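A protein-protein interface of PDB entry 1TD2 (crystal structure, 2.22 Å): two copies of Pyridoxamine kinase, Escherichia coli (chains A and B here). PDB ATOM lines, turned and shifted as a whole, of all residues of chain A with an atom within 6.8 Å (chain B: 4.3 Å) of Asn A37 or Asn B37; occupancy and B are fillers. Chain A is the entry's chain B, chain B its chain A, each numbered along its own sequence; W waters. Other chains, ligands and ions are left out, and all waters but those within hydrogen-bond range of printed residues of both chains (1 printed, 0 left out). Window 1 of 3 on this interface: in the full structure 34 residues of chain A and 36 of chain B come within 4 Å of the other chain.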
ATOM      1  N   ALA A   7      10.283 -11.480   1.701  1.00  0.00           N
ATOM      2  CA  ALA A   7      11.336 -12.417   1.304  1.00  0.00           C
ATOM      3  C   ALA A   7      11.401 -12.532  -0.216  1.00  0.00           C
ATOM      4  O   ALA A   7      10.448 -12.986  -0.878  1.00  0.00           O
ATOM      5  CB  ALA A   7      11.083 -13.819   1.963  1.00  0.00           C
ATOM      6  N   ILE A   8      12.536 -12.129  -0.768  1.00  0.00           N
ATOM      7  CA  ILE A   8      12.721 -12.152  -2.204  1.00  0.00           C
ATOM      8  C   ILE A   8      13.755 -13.186  -2.573  1.00  0.00           C
ATOM      9  O   ILE A   8      14.956 -12.922  -2.515  1.00  0.00           O
ATOM     10  CB  ILE A   8      13.198 -10.794  -2.733  1.00  0.00           C
ATOM     11  CG1 ILE A   8      12.457  -9.666  -2.011  1.00  0.00           C
ATOM     12  CG2 ILE A   8      12.982 -10.734  -4.255  1.00  0.00           C
ATOM     13  CD1 ILE A   8      13.024  -8.305  -2.287  1.00  0.00           C
ATOM     14  N   GLN A   9      13.271 -14.365  -2.940  1.00  0.00           N
ATOM     15  CA  GLN A   9      14.114 -15.466  -3.346  1.00  0.00           C
ATOM     16  C   GLN A   9      13.301 -16.500  -4.125  1.00  0.00           C
ATOM     17  O   GLN A   9      12.099 -16.339  -4.340  1.00  0.00           O
ATOM     18  CB  GLN A   9      14.812 -16.104  -2.134  1.00  0.00           C
ATOM     19  CG  GLN A   9      13.937 -16.386  -0.931  1.00  0.00           C
ATOM     20  CD  GLN A   9      14.745 -16.920   0.243  1.00  0.00           C
ATOM     21  OE1 GLN A   9      15.943 -17.160   0.125  1.00  0.00           O
ATOM     22  NE2 GLN A   9      14.092 -17.108   1.375  1.00  0.00           N
ATOM     23  N   SER A  10      13.990 -17.536  -4.580  1.00  0.00           N
ATOM     24  CA  SER A  10      13.391 -18.598  -5.363  1.00  0.00           C
ATOM     25  C   SER A  10      12.169 -19.287  -4.771  1.00  0.00           C
ATOM     26  O   SER A  10      11.892 -19.207  -3.571  1.00  0.00           O
ATOM     27  CB  SER A  10      14.451 -19.675  -5.638  1.00  0.00           C
ATOM     28  OG  SER A  10      15.076 -20.070  -4.425  1.00  0.00           O
ATOM     29  N   HIS A  11      11.455 -19.974  -5.650  1.00  0.00           N
ATOM     30  CA  HIS A  11      10.298 -20.793  -5.298  1.00  0.00           C
ATOM     31  C   HIS A  11      10.327 -22.038  -6.206  1.00  0.00           C
ATOM     32  O   HIS A  11      10.495 -21.926  -7.431  1.00  0.00           O
ATOM     33  CB  HIS A  11       8.972 -20.034  -5.507  1.00  0.00           C
ATOM     34  CG  HIS A  11       7.751 -20.891  -5.336  1.00  0.00           C
ATOM     35  ND1 HIS A  11       6.972 -21.297  -6.396  1.00  0.00           N
ATOM     36  CD2 HIS A  11       7.195 -21.444  -4.231  1.00  0.00           C
ATOM     37  CE1 HIS A  11       5.992 -22.066  -5.954  1.00  0.00           C
ATOM     38  NE2 HIS A  11       6.108 -22.172  -4.643  1.00  0.00           N
ATOM     39  N   VAL A  13       8.106 -25.525  -7.138  1.00  0.00           N
ATOM     40  CA  VAL A  13       6.766 -26.107  -6.967  1.00  0.00           C
ATOM     41  C   VAL A  13       6.913 -27.435  -6.217  1.00  0.00           C
ATOM     42  O   VAL A  13       6.230 -27.649  -5.216  1.00  0.00           O
ATOM     43  CB  VAL A  13       6.026 -26.279  -8.344  1.00  0.00           C
ATOM     44  CG1 VAL A  13       4.635 -26.853  -8.141  1.00  0.00           C
ATOM     45  CG2 VAL A  13       5.904 -24.911  -9.027  1.00  0.00           C
ATOM     46  N   ASN A  19      12.388 -19.678  -0.777  1.00  0.00           N
ATOM     47  CA  ASN A  19      11.089 -19.399  -0.155  1.00  0.00           C
ATOM     48  C   ASN A  19      10.306 -20.689   0.062  1.00  0.00           C
ATOM     49  O   ASN A  19       9.554 -20.822   1.039  1.00  0.00           O
ATOM     50  CB  ASN A  19      10.241 -18.436  -1.029  1.00  0.00           C
ATOM     51  CG  ASN A  19      10.486 -16.952  -0.687  1.00  0.00           C
ATOM     52  OD1 ASN A  19      10.927 -16.647   0.411  1.00  0.00           O
ATOM     53  ND2 ASN A  19      10.179 -16.031  -1.626  1.00  0.00           N
ATOM     54  N   SER A  20      10.470 -21.644  -0.847  1.00  0.00           N
ATOM     55  CA  SER A  20       9.744 -22.899  -0.699  1.00  0.00           C
ATOM     56  C   SER A  20      10.222 -23.664   0.533  1.00  0.00           C
ATOM     57  O   SER A  20       9.488 -24.490   1.085  1.00  0.00           O
ATOM     58  CB  SER A  20       9.868 -23.731  -1.969  1.00  0.00           C
ATOM     59  OG  SER A  20       9.397 -22.985  -3.087  1.00  0.00           O
ATOM     60  N   TRP A  34       6.032 -12.226   3.170  1.00  0.00           N
ATOM     61  CA  TRP A  34       5.466 -11.802   1.893  1.00  0.00           C
ATOM     62  C   TRP A  34       6.417 -12.430   0.880  1.00  0.00           C
ATOM     63  O   TRP A  34       7.463 -11.867   0.568  1.00  0.00           O
ATOM     64  CB  TRP A  34       5.492 -10.280   1.739  1.00  0.00           C
ATOM     65  CG  TRP A  34       4.811  -9.504   2.829  1.00  0.00           C
ATOM     66  CD1 TRP A  34       3.971  -9.989   3.809  1.00  0.00           C
ATOM     67  CD2 TRP A  34       4.948  -8.102   3.076  1.00  0.00           C
ATOM     68  NE1 TRP A  34       3.592  -8.966   4.655  1.00  0.00           N
ATOM     69  CE2 TRP A  34       4.177  -7.798   4.227  1.00  0.00           C
ATOM     70  CE3 TRP A  34       5.655  -7.068   2.437  1.00  0.00           C
ATOM     71  CZ2 TRP A  34       4.092  -6.495   4.758  1.00  0.00           C
ATOM     72  CZ3 TRP A  34       5.569  -5.767   2.968  1.00  0.00           C
ATOM     73  CH2 TRP A  34       4.791  -5.498   4.115  1.00  0.00           C
ATOM     74  N   PRO A  35       6.055 -13.592   0.327  1.00  0.00           N
ATOM     75  CA  PRO A  35       6.997 -14.181  -0.620  1.00  0.00           C
ATOM     76  C   PRO A  35       6.978 -13.610  -2.028  1.00  0.00           C
ATOM     77  O   PRO A  35       6.069 -13.892  -2.797  1.00  0.00           O
ATOM     78  CB  PRO A  35       6.631 -15.682  -0.606  1.00  0.00           C
ATOM     79  CG  PRO A  35       5.468 -15.807   0.419  1.00  0.00           C
ATOM     80  CD  PRO A  35       4.863 -14.436   0.468  1.00  0.00           C
ATOM     81  N   LEU A  36       7.986 -12.800  -2.351  1.00  0.00           N
ATOM     82  CA  LEU A  36       8.129 -12.257  -3.692  1.00  0.00           C
ATOM     83  C   LEU A  36       9.100 -13.238  -4.386  1.00  0.00           C
ATOM     84  O   LEU A  36      10.321 -13.116  -4.284  1.00  0.00           O
ATOM     85  CB  LEU A  36       8.708 -10.831  -3.635  1.00  0.00           C
ATOM     86  CG  LEU A  36       9.103 -10.141  -4.951  1.00  0.00           C
ATOM     87  CD1 LEU A  36       7.949 -10.279  -6.010  1.00  0.00           C
ATOM     88  CD2 LEU A  36       9.432  -8.664  -4.658  1.00  0.00           C
ATOM     89  N   ASN A  37       8.546 -14.226  -5.075  1.00  0.00           N
ATOM     90  CA  ASN A  37       9.355 -15.242  -5.754  1.00  0.00           C
ATOM     91  C   ASN A  37      10.203 -14.743  -6.942  1.00  0.00           C
ATOM     92  O   ASN A  37       9.687 -14.081  -7.851  1.00  0.00           O
ATOM     93  CB  ASN A  37       8.422 -16.375  -6.178  1.00  0.00           C
ATOM     94  CG  ASN A  37       7.640 -16.930  -5.002  1.00  0.00           C
ATOM     95  OD1 ASN A  37       6.512 -17.400  -5.148  1.00  0.00           O
ATOM     96  ND2 ASN A  37       8.247 -16.878  -3.820  1.00  0.00           N
ATOM     97  N   THR A  38      11.500 -15.067  -6.925  1.00  0.00           N
ATOM     98  CA  THR A  38      12.432 -14.646  -7.985  1.00  0.00           C
ATOM     99  C   THR A  38      12.394 -15.550  -9.214  1.00  0.00           C
ATOM    100  O   THR A  38      12.814 -15.168 -10.300  1.00  0.00           O
ATOM    101  CB  THR A  38      13.911 -14.587  -7.489  1.00  0.00           C
ATOM    102  OG1 THR A  38      14.323 -15.866  -6.963  1.00  0.00           O
ATOM    103  CG2 THR A  38      14.078 -13.491  -6.428  1.00  0.00           C
ATOM    104  N   VAL A  39      11.897 -16.762  -9.031  1.00  0.00           N
ATOM    105  CA  VAL A  39      11.788 -17.708 -10.127  1.00  0.00           C
ATOM    106  C   VAL A  39      10.680 -18.654  -9.700  1.00  0.00           C
ATOM    107  O   VAL A  39      10.265 -18.645  -8.541  1.00  0.00           O
ATOM    108  CB  VAL A  39      13.108 -18.572 -10.312  1.00  0.00           C
ATOM    109  CG1 VAL A  39      14.328 -17.703 -10.350  1.00  0.00           C
ATOM    110  CG2 VAL A  39      13.261 -19.562  -9.168  1.00  0.00           C
ATOM    111  N   GLN A  40      10.163 -19.426 -10.644  1.00  0.00           N
ATOM    112  CA  GLN A  40       9.215 -20.466 -10.298  1.00  0.00           C
ATOM    113  C   GLN A  40       9.746 -21.644 -11.081  1.00  0.00           C
ATOM    114  O   GLN A  40       9.553 -21.733 -12.293  1.00  0.00           O
ATOM    115  CB  GLN A  40       7.755 -20.173 -10.698  1.00  0.00           C
ATOM    116  CG  GLN A  40       6.830 -21.348 -10.262  1.00  0.00           C
ATOM    117  CD  GLN A  40       5.328 -21.035 -10.298  1.00  0.00           C
ATOM    118  OE1 GLN A  40       4.745 -20.818 -11.355  1.00  0.00           O
ATOM    119  NE2 GLN A  40       4.703 -21.027  -9.128  1.00  0.00           N
ATOM    120  N   VAL A  54      12.516 -17.420 -14.814  1.00  0.00           N
ATOM    121  CA  VAL A  54      13.046 -16.406 -13.911  1.00  0.00           C
ATOM    122  C   VAL A  54      12.126 -15.199 -13.987  1.00  0.00           C
ATOM    123  O   VAL A  54      11.814 -14.716 -15.087  1.00  0.00           O
ATOM    124  CB  VAL A  54      14.443 -15.942 -14.338  1.00  0.00           C
ATOM    125  CG1 VAL A  54      14.904 -14.761 -13.437  1.00  0.00           C
ATOM    126  CG2 VAL A  54      15.417 -17.114 -14.247  1.00  0.00           C
ATOM    127  N   MET A  55      11.664 -14.707 -12.845  1.00  0.00           N
ATOM    128  CA  MET A  55      10.778 -13.545 -12.908  1.00  0.00           C
ATOM    129  C   MET A  55      11.622 -12.401 -13.430  1.00  0.00           C
ATOM    130  O   MET A  55      12.773 -12.224 -13.007  1.00  0.00           O
ATOM    131  CB  MET A  55      10.208 -13.197 -11.534  1.00  0.00           C
ATOM    132  CG  MET A  55       9.330 -14.289 -10.927  1.00  0.00           C
ATOM    133  SD  MET A  55       7.897 -14.728 -11.968  1.00  0.00           S
ATOM    134  CE  MET A  55       8.519 -16.151 -12.695  1.00  0.00           C
ATOM    135  N   HIS A  59       9.501  -7.033 -12.847  1.00  0.00           N
ATOM    136  CA  HIS A  59       8.328  -7.599 -12.181  1.00  0.00           C
ATOM    137  C   HIS A  59       8.440  -7.379 -10.669  1.00  0.00           C
ATOM    138  O   HIS A  59       7.482  -6.969 -10.002  1.00  0.00           O
ATOM    139  CB  HIS A  59       8.250  -9.095 -12.455  1.00  0.00           C
ATOM    140  CG  HIS A  59       7.254  -9.804 -11.596  1.00  0.00           C
ATOM    141  ND1 HIS A  59       5.896  -9.750 -11.831  1.00  0.00           N
ATOM    142  CD2 HIS A  59       7.415 -10.577 -10.493  1.00  0.00           C
ATOM    143  CE1 HIS A  59       5.267 -10.460 -10.914  1.00  0.00           C
ATOM    144  NE2 HIS A  59       6.164 -10.973 -10.091  1.00  0.00           N
ATOM    145  N   LEU A  60       9.626  -7.660 -10.131  1.00  0.00           N
ATOM    146  CA  LEU A  60       9.878  -7.496  -8.702  1.00  0.00           C
ATOM    147  C   LEU A  60       9.646  -6.048  -8.249  1.00  0.00           C
ATOM    148  O   LEU A  60       9.101  -5.808  -7.166  1.00  0.00           O
ATOM    149  CB  LEU A  60      11.313  -7.906  -8.369  1.00  0.00           C
ATOM    150  CG  LEU A  60      11.850  -9.235  -8.920  1.00  0.00           C
ATOM    151  CD1 LEU A  60      13.274  -9.428  -8.390  1.00  0.00           C
ATOM    152  CD2 LEU A  60      10.949 -10.421  -8.532  1.00  0.00           C
ATOM    153  N   GLN A  89      18.381  -8.779 -11.245  1.00  0.00           N
ATOM    154  CA  GLN A  89      17.364  -8.772 -10.195  1.00  0.00           C
ATOM    155  C   GLN A  89      17.959  -8.066  -8.982  1.00  0.00           C
ATOM    156  O   GLN A  89      17.281  -7.281  -8.301  1.00  0.00           O
ATOM    157  CB  GLN A  89      16.978 -10.196  -9.808  1.00  0.00           C
ATOM    158  CG  GLN A  89      16.138 -10.916 -10.851  1.00  0.00           C
ATOM    159  CD  GLN A  89      15.578 -12.219 -10.335  1.00  0.00           C
ATOM    160  OE1 GLN A  89      14.521 -12.672 -10.782  1.00  0.00           O
ATOM    161  NE2 GLN A  89      16.278 -12.835  -9.393  1.00  0.00           N
ATOM    162  N   GLN B   9      -3.363 -22.462  -8.319  1.00  0.00           N
ATOM    163  CA  GLN B   9      -4.185 -21.290  -8.119  1.00  0.00           C
ATOM    164  C   GLN B   9      -3.227 -20.135  -7.810  1.00  0.00           C
ATOM    165  O   GLN B   9      -2.004 -20.303  -7.803  1.00  0.00           O
ATOM    166  CB  GLN B   9      -5.204 -21.523  -6.983  1.00  0.00           C
ATOM    167  CG  GLN B   9      -4.592 -22.088  -5.713  1.00  0.00           C
ATOM    168  CD  GLN B   9      -5.631 -22.399  -4.641  1.00  0.00           C
ATOM    169  OE1 GLN B   9      -6.817 -22.094  -4.797  1.00  0.00           O
ATOM    170  NE2 GLN B   9      -5.182 -22.999  -3.537  1.00  0.00           N
ATOM    171  N   HIS B  11      -1.179 -16.663  -6.336  1.00  0.00           N
ATOM    172  CA  HIS B  11      -0.217 -16.318  -5.311  1.00  0.00           C
ATOM    173  C   HIS B  11      -0.201 -14.778  -5.198  1.00  0.00           C
ATOM    174  O   HIS B  11      -0.123 -14.056  -6.205  1.00  0.00           O
ATOM    175  CB  HIS B  11       1.189 -16.828  -5.666  1.00  0.00           C
ATOM    176  CG  HIS B  11       2.256 -16.325  -4.739  1.00  0.00           C
ATOM    177  ND1 HIS B  11       2.175 -16.467  -3.371  1.00  0.00           N
ATOM    178  CD2 HIS B  11       3.406 -15.652  -4.978  1.00  0.00           C
ATOM    179  CE1 HIS B  11       3.227 -15.904  -2.807  1.00  0.00           C
ATOM    180  NE2 HIS B  11       3.989 -15.401  -3.758  1.00  0.00           N
ATOM    181  N   ASN B  19      -3.339 -19.803  -3.271  1.00  0.00           N
ATOM    182  CA  ASN B  19      -2.327 -20.578  -2.556  1.00  0.00           C
ATOM    183  C   ASN B  19      -1.802 -19.808  -1.368  1.00  0.00           C
ATOM    184  O   ASN B  19      -1.334 -20.410  -0.401  1.00  0.00           O
ATOM    185  CB  ASN B  19      -1.111 -20.888  -3.443  1.00  0.00           C
ATOM    186  CG  ASN B  19      -1.328 -22.065  -4.344  1.00  0.00           C
ATOM    187  OD1 ASN B  19      -2.041 -22.996  -3.994  1.00  0.00           O
ATOM    188  ND2 ASN B  19      -0.689 -22.046  -5.510  1.00  0.00           N
ATOM    189  N   PRO B  35       2.995 -25.789  -4.565  1.00  0.00           N
ATOM    190  CA  PRO B  35       2.238 -24.695  -5.167  1.00  0.00           C
ATOM    191  C   PRO B  35       2.643 -24.245  -6.559  1.00  0.00           C
ATOM    192  O   PRO B  35       3.694 -23.634  -6.746  1.00  0.00           O
ATOM    193  CB  PRO B  35       2.366 -23.547  -4.126  1.00  0.00           C
ATOM    194  CG  PRO B  35       3.384 -24.073  -3.053  1.00  0.00           C
ATOM    195  CD  PRO B  35       4.087 -25.259  -3.736  1.00  0.00           C
ATOM    196  N   LEU B  36       1.778 -24.527  -7.520  1.00  0.00           N
ATOM    197  CA  LEU B  36       1.982 -24.136  -8.906  1.00  0.00           C
ATOM    198  C   LEU B  36       1.116 -22.871  -9.065  1.00  0.00           C
ATOM    199  O   LEU B  36      -0.059 -22.942  -9.421  1.00  0.00           O
ATOM    200  CB  LEU B  36       1.518 -25.275  -9.839  1.00  0.00           C
ATOM    201  CG  LEU B  36       1.439 -25.063 -11.364  1.00  0.00           C
ATOM    202  CD1 LEU B  36       2.735 -24.421 -11.884  1.00  0.00           C
ATOM    203  CD2 LEU B  36       1.143 -26.414 -12.063  1.00  0.00           C
ATOM    204  N   ASN B  37       1.715 -21.720  -8.769  1.00  0.00           N
ATOM    205  CA  ASN B  37       1.035 -20.420  -8.811  1.00  0.00           C
ATOM    206  C   ASN B  37       0.594 -19.971 -10.212  1.00  0.00           C
ATOM    207  O   ASN B  37       1.401 -19.868 -11.122  1.00  0.00           O
ATOM    208  CB  ASN B  37       1.957 -19.375  -8.165  1.00  0.00           C
ATOM    209  CG  ASN B  37       2.386 -19.778  -6.747  1.00  0.00           C
ATOM    210  OD1 ASN B  37       3.478 -19.417  -6.267  1.00  0.00           O
ATOM    211  ND2 ASN B  37       1.523 -20.529  -6.071  1.00  0.00           N
ATOM    212  N   THR B  38      -0.697 -19.708 -10.375  1.00  0.00           N
ATOM    213  CA  THR B  38      -1.224 -19.297 -11.678  1.00  0.00           C
ATOM    214  C   THR B  38      -0.940 -17.826 -11.997  1.00  0.00           C
ATOM    215  O   THR B  38      -1.103 -17.392 -13.129  1.00  0.00           O
ATOM    216  CB  THR B  38      -2.745 -19.601 -11.782  1.00  0.00           C
ATOM    217  OG1 THR B  38      -3.459 -18.986 -10.695  1.00  0.00           O
ATOM    218  CG2 THR B  38      -2.975 -21.132 -11.755  1.00  0.00           C
ATOM    219  N   VAL B  39      -0.526 -17.070 -10.979  1.00  0.00           N
ATOM    220  CA  VAL B  39      -0.166 -15.658 -11.131  1.00  0.00           C
ATOM    221  C   VAL B  39       0.671 -15.281  -9.919  1.00  0.00           C
ATOM    222  O   VAL B  39       0.715 -16.024  -8.936  1.00  0.00           O
ATOM    223  CB  VAL B  39      -1.430 -14.680 -11.147  1.00  0.00           C
ATOM    224  CG1 VAL B  39      -2.489 -15.163 -12.114  1.00  0.00           C
ATOM    225  CG2 VAL B  39      -2.037 -14.556  -9.760  1.00  0.00           C
ATOM    226  N   GLN B  40       1.370 -14.156 -10.014  1.00  0.00           N
ATOM    227  CA  GLN B  40       2.093 -13.606  -8.879  1.00  0.00           C
ATOM    228  C   GLN B  40       1.652 -12.152  -8.869  1.00  0.00           C
ATOM    229  O   GLN B  40       2.101 -11.355  -9.687  1.00  0.00           O
ATOM    230  CB  GLN B  40       3.615 -13.677  -9.019  1.00  0.00           C
ATOM    231  CG  GLN B  40       4.313 -13.121  -7.746  1.00  0.00           C
ATOM    232  CD  GLN B  40       5.780 -13.535  -7.592  1.00  0.00           C
ATOM    233  OE1 GLN B  40       6.680 -12.958  -8.206  1.00  0.00           O
ATOM    234  NE2 GLN B  40       6.017 -14.541  -6.765  1.00  0.00           N
ATOM    235  N   MET B  55       0.739 -16.300 -15.099  1.00  0.00           N
ATOM    236  CA  MET B  55       1.717 -17.241 -15.626  1.00  0.00           C
ATOM    237  C   MET B  55       1.146 -17.754 -16.931  1.00  0.00           C
ATOM    238  O   MET B  55      -0.058 -17.999 -17.029  1.00  0.00           O
ATOM    239  CB  MET B  55       1.922 -18.413 -14.676  1.00  0.00           C
ATOM    240  CG  MET B  55       2.428 -18.017 -13.299  1.00  0.00           C
ATOM    241  SD  MET B  55       3.755 -16.789 -13.299  1.00  0.00           S
ATOM    242  CE  MET B  55       3.424 -15.995 -11.739  1.00  0.00           C
ATOM    243  N   LEU B  60       2.476 -23.647 -16.841  1.00  0.00           N
ATOM    244  CA  LEU B  60       1.882 -24.614 -15.932  1.00  0.00           C
ATOM    245  C   LEU B  60       2.227 -26.024 -16.386  1.00  0.00           C
ATOM    246  O   LEU B  60       2.573 -26.891 -15.572  1.00  0.00           O
ATOM    247  CB  LEU B  60       0.365 -24.436 -15.900  1.00  0.00           C
ATOM    248  CG  LEU B  60      -0.097 -23.031 -15.487  1.00  0.00           C
ATOM    249  CD1 LEU B  60      -1.637 -23.033 -15.315  1.00  0.00           C
ATOM    250  CD2 LEU B  60       0.598 -22.602 -14.176  1.00  0.00           C
HETATM  251  O   HOH W   1       5.927 -17.101 -10.687  1.00  0.00           O
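A ring nitrogen (NE2) of His B11 lies within hydrogen-bond range of the backbone carbonyl oxygen of Pro A35. N of Asn B37 sits close to NE2 of Gln A40 (3.1 Å). The side-chain amide nitrogen of Gln B40 lies close to the backbone NH of Asn A37, at 3.1 Å. OE1 of Gln B40 lies within hydrogen-bond range of NE2 of His A59.
The backbone carbonyl oxygen (O) of Val B39 sits at hydrogen-bond distance from the backbone NH (N) of His B11. ND2 of Asn B19 sits close to ND2 of Asn B37. N of Leu A36 lies within hydrogen-bond range of O of Ala A7 (2.9 Å). N of Gln A9 lies within hydrogen-bond range of O of Leu A36, at 3.5 Å. The backbone carbonyl oxygen of Val A39 is in hydrogen-bond range of the backbone NH of His A11, at 3.4 Å. ND2 of Asn A37 lies close to ND2 of Asn A19 (3.0 Å).
Among the printed residues, merely in contact across the chains: His A11 with Pro B35 (2.9 Å), His A11 with Asn B37 (3.7 Å), Val A13 with Pro B35 (3.4 Å), Val A13 with Leu B36 (3.7 Å), Leu A36 with Gln B40 (3.7 Å), Asn A37 with His B11 (3.5 Å), Asn A37 with Asn B37 (3.8 Å) and Gln A40 with Pro B35 (3.7 Å).
Asn A37 touches just these residues of chain B: His B11, Asn B37 and Gln B40. Asn B37 touches three residues of chain A. Of the printed residues of chain B, Val A13 touches Pro B35 (3.4 Å) and Leu B36 (3.7 Å). Of the printed residues of chain A, His B11 touches Pro A35 and Asn A37. Of the printed residues of chain B, His A59 touches Gln B40 (2.8 Å). Printed residues of chain B within 4 Å of His A11: Pro B35 and Asn B37. Of the printed residues of chain B, Gln A40 touches Pro B35 (3.7 Å) and Asn B37 (3.1 Å). Leu A60 touches none of the printed residues of chain B. The nearest printed residue of chain B that does not touch Asn A37 is Pro B35 (7.0 Å). The nearest printed residue of chain A that does not touch Pro B35 is Ser A20 (5.8 Å).
Of the 11 printed residues of chain B, 5 touch a printed residue of chain A. Along chain B the printed residues that touch a printed residue of chain A span positions 11 to 40. Hydrophobic or aromatic side chains of chain A that line the printed part of chain B: His A11, Val A13, Pro A35, Leu A36 and His A59. Along chain A the printed residues that touch a printed residue of chain B span positions 11 to 59. Among the printed residues, no Asp or Glu carboxylate lies within 4 Å of a Lys or Arg side-chain nitrogen of the other chain.
His A11 touches Pro B35, and with the chains exchanged Pro A35 touches His B11. Leu A36 touches Gln B40, but with the chains exchanged Gln A40 does not touch Leu B36 (4.03 Å). Asn A37 touches Gln B40, and with the chains exchanged Gln A40 touches Asn B37. Gln A40 touches Pro B35, but with the chains exchanged Pro A35 does not touch Gln B40 (4.02 Å).
Water W1 bridges SD of Met A55 (3.3 Å) and SD of Met B55 (3.4 Å).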
